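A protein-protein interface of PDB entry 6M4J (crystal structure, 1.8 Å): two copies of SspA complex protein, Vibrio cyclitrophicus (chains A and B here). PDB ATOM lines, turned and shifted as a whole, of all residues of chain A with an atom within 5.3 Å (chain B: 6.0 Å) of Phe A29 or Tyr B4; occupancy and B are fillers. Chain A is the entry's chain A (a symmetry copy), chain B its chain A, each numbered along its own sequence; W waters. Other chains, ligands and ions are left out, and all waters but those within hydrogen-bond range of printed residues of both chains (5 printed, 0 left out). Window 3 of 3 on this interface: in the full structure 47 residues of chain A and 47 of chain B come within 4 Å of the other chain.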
ATOM      1  N   TRP A  24       6.986 -16.298  19.658  1.00  0.00           N
ATOM      2  CA  TRP A  24       7.270 -17.313  18.647  1.00  0.00           C
ATOM      3  C   TRP A  24       7.357 -16.760  17.268  1.00  0.00           C
ATOM      4  O   TRP A  24       7.407 -17.517  16.300  1.00  0.00           O
ATOM      5  CB  TRP A  24       6.213 -18.404  18.678  1.00  0.00           C
ATOM      6  CG  TRP A  24       6.080 -19.024  20.036  1.00  0.00           C
ATOM      7  CD1 TRP A  24       5.088 -18.783  20.983  1.00  0.00           C
ATOM      8  CD2 TRP A  24       7.008 -19.961  20.672  1.00  0.00           C
ATOM      9  NE1 TRP A  24       5.317 -19.517  22.120  1.00  0.00           N
ATOM     10  CE2 TRP A  24       6.456 -20.244  21.999  1.00  0.00           C
ATOM     11  CE3 TRP A  24       8.187 -20.592  20.282  1.00  0.00           C
ATOM     12  CZ2 TRP A  24       7.077 -21.119  22.879  1.00  0.00           C
ATOM     13  CZ3 TRP A  24       8.806 -21.471  21.180  1.00  0.00           C
ATOM     14  CH2 TRP A  24       8.265 -21.724  22.445  1.00  0.00           C
ATOM     15  N   GLN A  25       7.414 -15.439  17.181  1.00  0.00           N
ATOM     16  CA  GLN A  25       7.554 -14.765  15.911  1.00  0.00           C
ATOM     17  C   GLN A  25       9.022 -14.537  15.569  1.00  0.00           C
ATOM     18  O   GLN A  25       9.510 -15.040  14.569  1.00  0.00           O
ATOM     19  CB  GLN A  25       6.758 -13.455  15.913  1.00  0.00           C
ATOM     20  CG  GLN A  25       5.300 -13.579  16.377  1.00  0.00           C
ATOM     21  CD  GLN A  25       4.349 -14.158  15.337  1.00  0.00           C
ATOM     22  OE1 GLN A  25       3.143 -14.242  15.579  1.00  0.00           O
ATOM     23  NE2 GLN A  25       4.876 -14.557  14.184  1.00  0.00           N
ATOM     24  N   SER A  26       9.720 -13.785  16.411  1.00  0.00           N
ATOM     25  CA  SER A  26      11.131 -13.508  16.180  1.00  0.00           C
ATOM     26  C   SER A  26      12.047 -13.907  17.338  1.00  0.00           C
ATOM     27  O   SER A  26      13.234 -14.145  17.121  1.00  0.00           O
ATOM     28  CB  SER A  26      11.352 -12.033  15.815  1.00  0.00           C
ATOM     29  OG  SER A  26      10.856 -11.204  16.838  1.00  0.00           O
ATOM     30  N   ASP A  27      11.536 -13.994  18.566  1.00  0.00           N
ATOM     31  CA  ASP A  27      12.380 -14.414  19.711  1.00  0.00           C
ATOM     32  C   ASP A  27      12.852 -15.878  19.630  1.00  0.00           C
ATOM     33  O   ASP A  27      14.027 -16.171  19.849  1.00  0.00           O
ATOM     34  CB  ASP A  27      11.675 -14.186  21.046  1.00  0.00           C
ATOM     35  CG  ASP A  27      11.494 -12.718  21.380  1.00  0.00           C
ATOM     36  OD1 ASP A  27      12.091 -11.842  20.711  1.00  0.00           O
ATOM     37  OD2 ASP A  27      10.740 -12.443  22.335  1.00  0.00           O
ATOM     38  N   SER A  28      11.919 -16.782  19.336  1.00  0.00           N
ATOM     39  CA  SER A  28      12.197 -18.206  19.204  1.00  0.00           C
ATOM     40  C   SER A  28      11.405 -18.700  18.019  1.00  0.00           C
ATOM     41  O   SER A  28      10.193 -18.734  18.079  1.00  0.00           O
ATOM     42  CB  SER A  28      11.761 -18.931  20.473  1.00  0.00           C
ATOM     43  OG  SER A  28      11.987 -20.326  20.383  1.00  0.00           O
ATOM     44  N   PHE A  29      12.066 -19.032  16.928  1.00  0.00           N
ATOM     45  CA  PHE A  29      11.323 -19.182  15.699  1.00  0.00           C
ATOM     46  C   PHE A  29      11.705 -20.457  14.974  1.00  0.00           C
ATOM     47  O   PHE A  29      11.508 -20.561  13.764  1.00  0.00           O
ATOM     48  CB  PHE A  29      11.611 -17.971  14.815  1.00  0.00           C
ATOM     49  CG  PHE A  29      13.078 -17.712  14.627  1.00  0.00           C
ATOM     50  CD1 PHE A  29      13.804 -16.949  15.539  1.00  0.00           C
ATOM     51  CD2 PHE A  29      13.740 -18.258  13.547  1.00  0.00           C
ATOM     52  CE1 PHE A  29      15.170 -16.751  15.374  1.00  0.00           C
ATOM     53  CE2 PHE A  29      15.093 -18.044  13.363  1.00  0.00           C
ATOM     54  CZ  PHE A  29      15.812 -17.292  14.278  1.00  0.00           C
ATOM     55  N   ALA A  30      12.250 -21.439  15.690  1.00  0.00           N
ATOM     56  CA  ALA A  30      12.726 -22.668  15.030  1.00  0.00           C
ATOM     57  C   ALA A  30      11.618 -23.457  14.320  1.00  0.00           C
ATOM     58  O   ALA A  30      10.446 -23.348  14.671  1.00  0.00           O
ATOM     59  CB  ALA A  30      13.424 -23.569  16.039  1.00  0.00           C
ATOM     60  N   ASN A  31      11.998 -24.271  13.336  1.00  0.00           N
ATOM     61  CA  ASN A  31      11.083 -25.262  12.795  1.00  0.00           C
ATOM     62  C   ASN A  31      10.962 -26.352  13.845  1.00  0.00           C
ATOM     63  O   ASN A  31      11.954 -26.933  14.233  1.00  0.00           O
ATOM     64  CB  ASN A  31      11.635 -25.850  11.488  1.00  0.00           C
ATOM     65  CG  ASN A  31      10.625 -26.728  10.759  1.00  0.00           C
ATOM     66  OD1 ASN A  31       9.899 -27.511  11.372  1.00  0.00           O
ATOM     67  ND2 ASN A  31      10.572 -26.588   9.429  1.00  0.00           N
ATOM     68  N   HIS A  36      17.234 -29.479  17.554  1.00  0.00           N
ATOM     69  CA  HIS A  36      17.978 -28.717  18.549  1.00  0.00           C
ATOM     70  C   HIS A  36      17.052 -28.090  19.543  1.00  0.00           C
ATOM     71  O   HIS A  36      15.846 -28.305  19.475  1.00  0.00           O
ATOM     72  CB  HIS A  36      18.884 -27.695  17.878  1.00  0.00           C
ATOM     73  CG  HIS A  36      18.190 -26.863  16.849  1.00  0.00           C
ATOM     74  ND1 HIS A  36      17.234 -25.971  17.167  1.00  0.00           N
ATOM     75  CD2 HIS A  36      18.336 -26.815  15.467  1.00  0.00           C
ATOM     76  CE1 HIS A  36      16.796 -25.372  16.041  1.00  0.00           C
ATOM     77  NE2 HIS A  36      17.464 -25.896  15.002  1.00  0.00           N
ATOM     78  N   GLU A  38      15.897 -25.103  20.254  1.00  0.00           N
ATOM     79  CA  GLU A  38      14.854 -24.153  19.937  1.00  0.00           C
ATOM     80  C   GLU A  38      13.626 -24.881  19.420  1.00  0.00           C
ATOM     81  O   GLU A  38      12.498 -24.480  19.716  1.00  0.00           O
ATOM     82  CB  GLU A  38      15.334 -23.068  18.983  1.00  0.00           C
ATOM     83  CG  GLU A  38      16.260 -22.037  19.623  1.00  0.00           C
ATOM     84  CD  GLU A  38      15.638 -21.304  20.801  1.00  0.00           C
ATOM     85  OE1 GLU A  38      16.244 -21.317  21.891  1.00  0.00           O
ATOM     86  OE2 GLU A  38      14.546 -20.732  20.654  1.00  0.00           O
ATOM     87  N   THR B   2      21.651 -18.128  19.548  1.00  0.00           N
ATOM     88  CA  THR B   2      22.784 -18.364  20.478  1.00  0.00           C
ATOM     89  C   THR B   2      23.493 -19.697  20.253  1.00  0.00           C
ATOM     90  O   THR B   2      23.614 -20.513  21.180  1.00  0.00           O
ATOM     91  CB  THR B   2      22.314 -18.245  21.922  1.00  0.00           C
ATOM     92  N   LYS B   3      23.917 -19.940  19.021  1.00  0.00           N
ATOM     93  CA  LYS B   3      23.574 -19.068  17.936  1.00  0.00           C
ATOM     94  C   LYS B   3      22.904 -19.895  16.843  1.00  0.00           C
ATOM     95  O   LYS B   3      23.323 -20.986  16.469  1.00  0.00           O
ATOM     96  CB  LYS B   3      24.799 -18.291  17.429  1.00  0.00           C
ATOM     97  CG  LYS B   3      24.489 -16.950  16.764  1.00  0.00           C
ATOM     98  CD  LYS B   3      23.659 -16.034  17.654  1.00  0.00           C
ATOM     99  CE  LYS B   3      22.392 -15.608  16.926  1.00  0.00           C
ATOM    100  NZ  LYS B   3      21.182 -16.355  17.364  1.00  0.00           N
ATOM    101  N   TYR B   4      21.916 -19.272  16.260  1.00  0.00           N
ATOM    102  CA  TYR B   4      21.052 -19.963  15.317  1.00  0.00           C
ATOM    103  C   TYR B   4      21.633 -19.920  13.923  1.00  0.00           C
ATOM    104  O   TYR B   4      21.802 -18.854  13.355  1.00  0.00           O
ATOM    105  CB  TYR B   4      19.686 -19.271  15.336  1.00  0.00           C
ATOM    106  CG  TYR B   4      18.550 -19.915  14.562  1.00  0.00           C
ATOM    107  CD1 TYR B   4      18.334 -19.621  13.227  1.00  0.00           C
ATOM    108  CD2 TYR B   4      17.676 -20.770  15.188  1.00  0.00           C
ATOM    109  CE1 TYR B   4      17.303 -20.204  12.544  1.00  0.00           C
ATOM    110  CE2 TYR B   4      16.639 -21.345  14.503  1.00  0.00           C
ATOM    111  CZ  TYR B   4      16.460 -21.061  13.180  1.00  0.00           C
ATOM    112  OH  TYR B   4      15.407 -21.607  12.490  1.00  0.00           O
ATOM    113  N   PHE B   5      21.906 -21.089  13.372  1.00  0.00           N
ATOM    114  CA  PHE B   5      22.398 -21.204  12.009  1.00  0.00           C
ATOM    115  C   PHE B   5      21.541 -22.212  11.244  1.00  0.00           C
ATOM    116  O   PHE B   5      22.049 -23.086  10.544  1.00  0.00           O
ATOM    117  CB  PHE B   5      23.846 -21.688  12.030  1.00  0.00           C
ATOM    118  CG  PHE B   5      24.851 -20.620  12.336  1.00  0.00           C
ATOM    119  CD1 PHE B   5      25.503 -19.976  11.315  1.00  0.00           C
ATOM    120  CD2 PHE B   5      25.161 -20.286  13.642  1.00  0.00           C
ATOM    121  CE1 PHE B   5      26.431 -18.999  11.598  1.00  0.00           C
ATOM    122  CE2 PHE B   5      26.095 -19.318  13.931  1.00  0.00           C
ATOM    123  CZ  PHE B   5      26.745 -18.675  12.903  1.00  0.00           C
ATOM    124  N   ASP B   6      20.231 -22.103  11.403  1.00  0.00           N
ATOM    125  CA  ASP B   6      19.316 -23.061  10.806  1.00  0.00           C
ATOM    126  C   ASP B   6      18.242 -22.334  10.020  1.00  0.00           C
ATOM    127  O   ASP B   6      17.080 -22.713  10.068  1.00  0.00           O
ATOM    128  CB  ASP B   6      18.671 -23.881  11.911  1.00  0.00           C
ATOM    129  CG  ASP B   6      18.255 -25.259  11.450  1.00  0.00           C
ATOM    130  OD1 ASP B   6      17.431 -25.886  12.046  1.00  0.00           O
ATOM    131  OD2 ASP B   6      18.691 -25.761  10.457  1.00  0.00           O
ATOM    132  N   TYR B   7      18.633 -21.273   9.319  1.00  0.00           N
ATOM    133  CA  TYR B   7      17.678 -20.490   8.560  1.00  0.00           C
ATOM    134  C   TYR B   7      17.000 -21.259   7.427  1.00  0.00           C
ATOM    135  O   TYR B   7      15.914 -20.883   7.054  1.00  0.00           O
ATOM    136  CB  TYR B   7      18.283 -19.156   8.046  1.00  0.00           C
ATOM    137  CG  TYR B   7      18.750 -18.233   9.142  1.00  0.00           C
ATOM    138  CD1 TYR B   7      20.047 -18.310   9.633  1.00  0.00           C
ATOM    139  CD2 TYR B   7      17.890 -17.303   9.713  1.00  0.00           C
ATOM    140  CE1 TYR B   7      20.479 -17.494  10.648  1.00  0.00           C
ATOM    141  CE2 TYR B   7      18.325 -16.480  10.742  1.00  0.00           C
ATOM    142  CZ  TYR B   7      19.624 -16.582  11.202  1.00  0.00           C
ATOM    143  OH  TYR B   7      20.054 -15.775  12.246  1.00  0.00           O
ATOM    144  N   ALA B   9      15.704 -23.975   7.672  1.00  0.00           N
ATOM    145  CA  ALA B   9      14.554 -24.619   8.321  1.00  0.00           C
ATOM    146  C   ALA B   9      13.441 -23.651   8.694  1.00  0.00           C
ATOM    147  O   ALA B   9      12.266 -23.978   8.522  1.00  0.00           O
ATOM    148  CB  ALA B   9      14.980 -25.407   9.553  1.00  0.00           C
ATOM    149  N   SER B  10      13.799 -22.483   9.219  1.00  0.00           N
ATOM    150  CA  SER B  10      12.830 -21.402   9.392  1.00  0.00           C
ATOM    151  C   SER B  10      13.522 -20.110   9.716  1.00  0.00           C
ATOM    152  O   SER B  10      14.683 -20.105  10.130  1.00  0.00           O
ATOM    153  CB  SER B  10      11.820 -21.715  10.487  1.00  0.00           C
ATOM    154  OG  SER B  10      10.762 -20.766  10.420  1.00  0.00           O
ATOM    155  N   THR B  11      12.798 -19.017   9.561  1.00  0.00           N
ATOM    156  CA  THR B  11      13.402 -17.728   9.727  1.00  0.00           C
ATOM    157  C   THR B  11      12.595 -16.900  10.672  1.00  0.00           C
ATOM    158  O   THR B  11      11.437 -17.180  10.937  1.00  0.00           O
ATOM    159  CB  THR B  11      13.496 -16.969   8.400  1.00  0.00           C
ATOM    160  OG1 THR B  11      12.189 -16.829   7.847  1.00  0.00           O
ATOM    161  CG2 THR B  11      14.340 -17.757   7.452  1.00  0.00           C
ATOM    162  N   PRO B  12      13.214 -15.851  11.199  1.00  0.00           N
ATOM    163  CA  PRO B  12      12.539 -14.985  12.154  1.00  0.00           C
ATOM    164  C   PRO B  12      11.658 -13.934  11.491  1.00  0.00           C
ATOM    165  O   PRO B  12      12.079 -13.273  10.551  1.00  0.00           O
ATOM    166  CB  PRO B  12      13.698 -14.287  12.857  1.00  0.00           C
ATOM    167  CG  PRO B  12      14.799 -14.253  11.839  1.00  0.00           C
ATOM    168  CD  PRO B  12      14.582 -15.398  10.882  1.00  0.00           C
ATOM    169  N   VAL B  13      10.460 -13.733  12.012  1.00  0.00           N
ATOM    170  CA  VAL B  13       9.550 -12.766  11.409  1.00  0.00           C
ATOM    171  C   VAL B  13      10.084 -11.346  11.550  1.00  0.00           C
ATOM    172  O   VAL B  13      10.390 -10.916  12.659  1.00  0.00           O
ATOM    173  CB  VAL B  13       8.198 -12.832  12.103  1.00  0.00           C
ATOM    174  CG1 VAL B  13       7.256 -11.804  11.533  1.00  0.00           C
ATOM    175  CG2 VAL B  13       7.594 -14.214  11.931  1.00  0.00           C
ATOM    176  N   LYS B 206       4.787 -18.095  10.067  1.00  0.00           N
ATOM    177  CA  LYS B 206       4.419 -19.485   9.851  1.00  0.00           C
ATOM    178  C   LYS B 206       2.917 -19.599   9.567  1.00  0.00           C
ATOM    179  O   LYS B 206       2.113 -18.734   9.969  1.00  0.00           O
ATOM    180  CB  LYS B 206       4.817 -20.352  11.059  1.00  0.00           C
ATOM    181  CG  LYS B 206       6.316 -20.618  11.130  1.00  0.00           C
ATOM    182  CD  LYS B 206       6.705 -21.429  12.364  1.00  0.00           C
ATOM    183  CE  LYS B 206       8.229 -21.547  12.482  1.00  0.00           C
ATOM    184  NZ  LYS B 206       8.889 -20.244  12.822  1.00  0.00           N
ATOM    185  N   GLN B 262      26.117 -11.662  10.295  1.00  0.00           N
ATOM    186  CA  GLN B 262      26.255 -13.053  10.712  1.00  0.00           C
ATOM    187  C   GLN B 262      27.011 -13.853   9.675  1.00  0.00           C
ATOM    188  O   GLN B 262      27.849 -14.690  10.035  1.00  0.00           O
ATOM    189  CB  GLN B 262      24.935 -13.755  11.033  1.00  0.00           C
ATOM    190  CG  GLN B 262      25.133 -15.171  11.621  1.00  0.00           C
ATOM    191  CD  GLN B 262      23.841 -15.813  12.026  1.00  0.00           C
ATOM    192  OE1 GLN B 262      22.802 -15.168  12.052  1.00  0.00           O
ATOM    193  NE2 GLN B 262      23.899 -17.082  12.360  1.00  0.00           N
ATOM    194  N   ASN B 305      28.588 -23.404  19.702  1.00  0.00           N
ATOM    195  CA  ASN B 305      27.309 -23.873  20.127  1.00  0.00           C
ATOM    196  C   ASN B 305      26.232 -23.446  19.134  1.00  0.00           C
ATOM    197  O   ASN B 305      25.282 -22.791  19.513  1.00  0.00           O
ATOM    198  CB  ASN B 305      27.032 -23.319  21.510  1.00  0.00           C
ATOM    199  CG  ASN B 305      25.880 -24.014  22.199  1.00  0.00           C
ATOM    200  OD1 ASN B 305      25.276 -24.940  21.649  1.00  0.00           O
ATOM    201  ND2 ASN B 305      25.560 -23.568  23.415  1.00  0.00           N
ATOM    202  N   TRP B 306      26.373 -23.827  17.866  1.00  0.00           N
ATOM    203  CA  TRP B 306      25.401 -23.432  16.836  1.00  0.00           C
ATOM    204  C   TRP B 306      24.231 -24.352  16.699  1.00  0.00           C
ATOM    205  O   TRP B 306      24.395 -25.580  16.766  1.00  0.00           O
ATOM    206  CB  TRP B 306      26.087 -23.352  15.491  1.00  0.00           C
ATOM    207  CG  TRP B 306      27.200 -22.351  15.459  1.00  0.00           C
ATOM    208  CD1 TRP B 306      27.566 -21.450  16.451  1.00  0.00           C
ATOM    209  CD2 TRP B 306      28.109 -22.091  14.352  1.00  0.00           C
ATOM    210  NE1 TRP B 306      28.624 -20.682  16.044  1.00  0.00           N
ATOM    211  CE2 TRP B 306      29.005 -21.027  14.801  1.00  0.00           C
ATOM    212  CE3 TRP B 306      28.284 -22.634  13.087  1.00  0.00           C
ATOM    213  CZ2 TRP B 306      30.004 -20.532  14.002  1.00  0.00           C
ATOM    214  CZ3 TRP B 306      29.311 -22.127  12.282  1.00  0.00           C
ATOM    215  CH2 TRP B 306      30.142 -21.091  12.728  1.00  0.00           C
ATOM    216  N   LEU B 307      23.044 -23.784  16.478  1.00  0.00           N
ATOM    217  CA  LEU B 307      21.896 -24.610  16.157  1.00  0.00           C
ATOM    218  C   LEU B 307      21.874 -24.784  14.665  1.00  0.00           C
ATOM    219  O   LEU B 307      21.707 -23.819  13.890  1.00  0.00           O
ATOM    220  CB  LEU B 307      20.611 -23.968  16.638  1.00  0.00           C
ATOM    221  CG  LEU B 307      20.779 -23.423  18.051  1.00  0.00           C
ATOM    222  CD1 LEU B 307      19.600 -22.539  18.402  1.00  0.00           C
ATOM    223  CD2 LEU B 307      20.941 -24.548  19.065  1.00  0.00           C
ATOM    224  N   SER B 342      23.202 -22.921   7.844  1.00  0.00           N
ATOM    225  CA  SER B 342      22.518 -21.964   6.968  1.00  0.00           C
ATOM    226  C   SER B 342      22.402 -20.562   7.565  1.00  0.00           C
ATOM    227  O   SER B 342      22.401 -20.394   8.785  1.00  0.00           O
ATOM    228  CB  SER B 342      21.164 -22.506   6.510  1.00  0.00           C
ATOM    229  OG  SER B 342      20.358 -22.889   7.591  1.00  0.00           O
HETATM  230  O   HOH W   1       8.923 -10.183  15.092  1.00  0.00           O
HETATM  231  O   HOH W   2       7.431 -17.641  13.369  1.00  0.00           O
HETATM  232  O   HOH W   3       7.736 -20.086  15.368  1.00  0.00           O
HETATM  233  O   HOH W   4      15.040 -24.279  13.085  1.00  0.00           O
HETATM  234  O   HOH W   5       4.986 -16.906  12.698  1.00  0.00           O
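OD1 of Asp B6 sits at hydrogen-bond distance from NE2 of His A36, at 3.0 Å. ND2 of Asn A31 is in hydrogen-bond range of O of Ala B9, 3.2 Å away. The backbone carbonyl oxygen (O) of Phe A29 is in hydrogen-bond range of the side-chain hydroxyl (OG) of Ser B10, at 3.4 Å. The backbone NH of Val B13 sits at hydrogen-bond distance from the backbone carbonyl oxygen of Gln A25 (3.0 Å). NZ of Lys B206 lies within hydrogen-bond range of O of Phe A29 (2.8 Å).
Water W3 bridges O of Trp A24 (2.8 Å) and NZ of Lys B206 (2.8 Å). Water W4 lies within hydrogen-bond range of the side-chain hydroxyl of Tyr B4 (2.8 Å), the backbone NH of Asn A31 (3.1 Å), the side-chain carboxylate of Asp B6 (3.1 Å) and a ring nitrogen (NE2) of His A36 (3.5 Å). Water W5 bridges the side-chain amide nitrogen of Gln A25 (2.8 Å) and the backbone NH of Lys B206 (2.9 Å). Water W1 bridges OG of Ser A26 (2.8 Å) and O of Val B13 (2.9 Å). Water W2 bridges the backbone carbonyl oxygen of Trp A24 and the side-chain amino group of Lys B206.
OH of Tyr B4 is in hydrogen-bond range of O of Asp B6, 3.1 Å away. The backbone NH of Phe B5 lies within hydrogen-bond range of the backbone carbonyl oxygen of Leu B307. N of Asp B6 lies within hydrogen-bond range of O of Leu B307, at 3.4 Å. The side-chain hydroxyl of Ser B10 is in hydrogen-bond range of the side-chain amino group of Lys B206, 3.1 Å away. OG of Ser A28 lies within hydrogen-bond range of OE2 of Glu A38 (2.6 Å). ND1 of His A36 lies close to N of Glu A38.
Of the 10 printed residues of chain A, 7 touch a printed residue of chain B. Hydrophobic or aromatic side chains of chain A within 4 Å of the printed part of chain B: Phe A29 and His A36. Printed residues of chain B that touch a printed residue of chain A: Tyr B4, Asp B6, Ala B9, Ser B10, Thr B11, Pro B12, Val B13, Lys B206 and Leu B307. Among the printed residues, 15 pairs touch across the chains.
Among the printed residues, pairs that only touch across the chains: Phe A29 with Tyr B4 (3.2 Å), Phe A29 with Thr B11 (3.4 Å), Phe A29 with Pro B12 (3.4 Å), Ser A26 with Val B13 (3.5 Å), Glu A38 with Leu B307 (3.6 Å), Ala A30 with Lys B206 (3.6 Å), His A36 with Leu B307 (3.8 Å), Asn A31 with Ser B10 (3.8 Å), Ala A30 with Tyr B4 (3.8 Å) and Gln A25 with Pro B12 (3.9 Å).
Phe A29 touches just these residues of chain B: Tyr B4, Ser B10, Thr B11, Pro B12 and Lys B206. Of the printed residues of chain B, Asn A31 touches Ala B9 and Ser B10. Printed residues of chain B within 4 Å of Glu A38: Leu B307. Printed residues of chain A within 4 Å of Tyr B4: Phe A29 and Ala A30. Of the printed residues of chain A, Ala B9 touches Asn A31 (3.2 Å). Printed residues of chain A within 4 Å of Thr B11: Phe A29. Of the printed residues of chain A, Val B13 touches Gln A25 and Ser A26. The nearest residue of chain A that does not touch Tyr B4 is His A36 (4.3 Å). The nearest printed residue of chain A that does not touch Pro B12 is Ser A26 (4.3 Å).
No position is printed for both chains.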
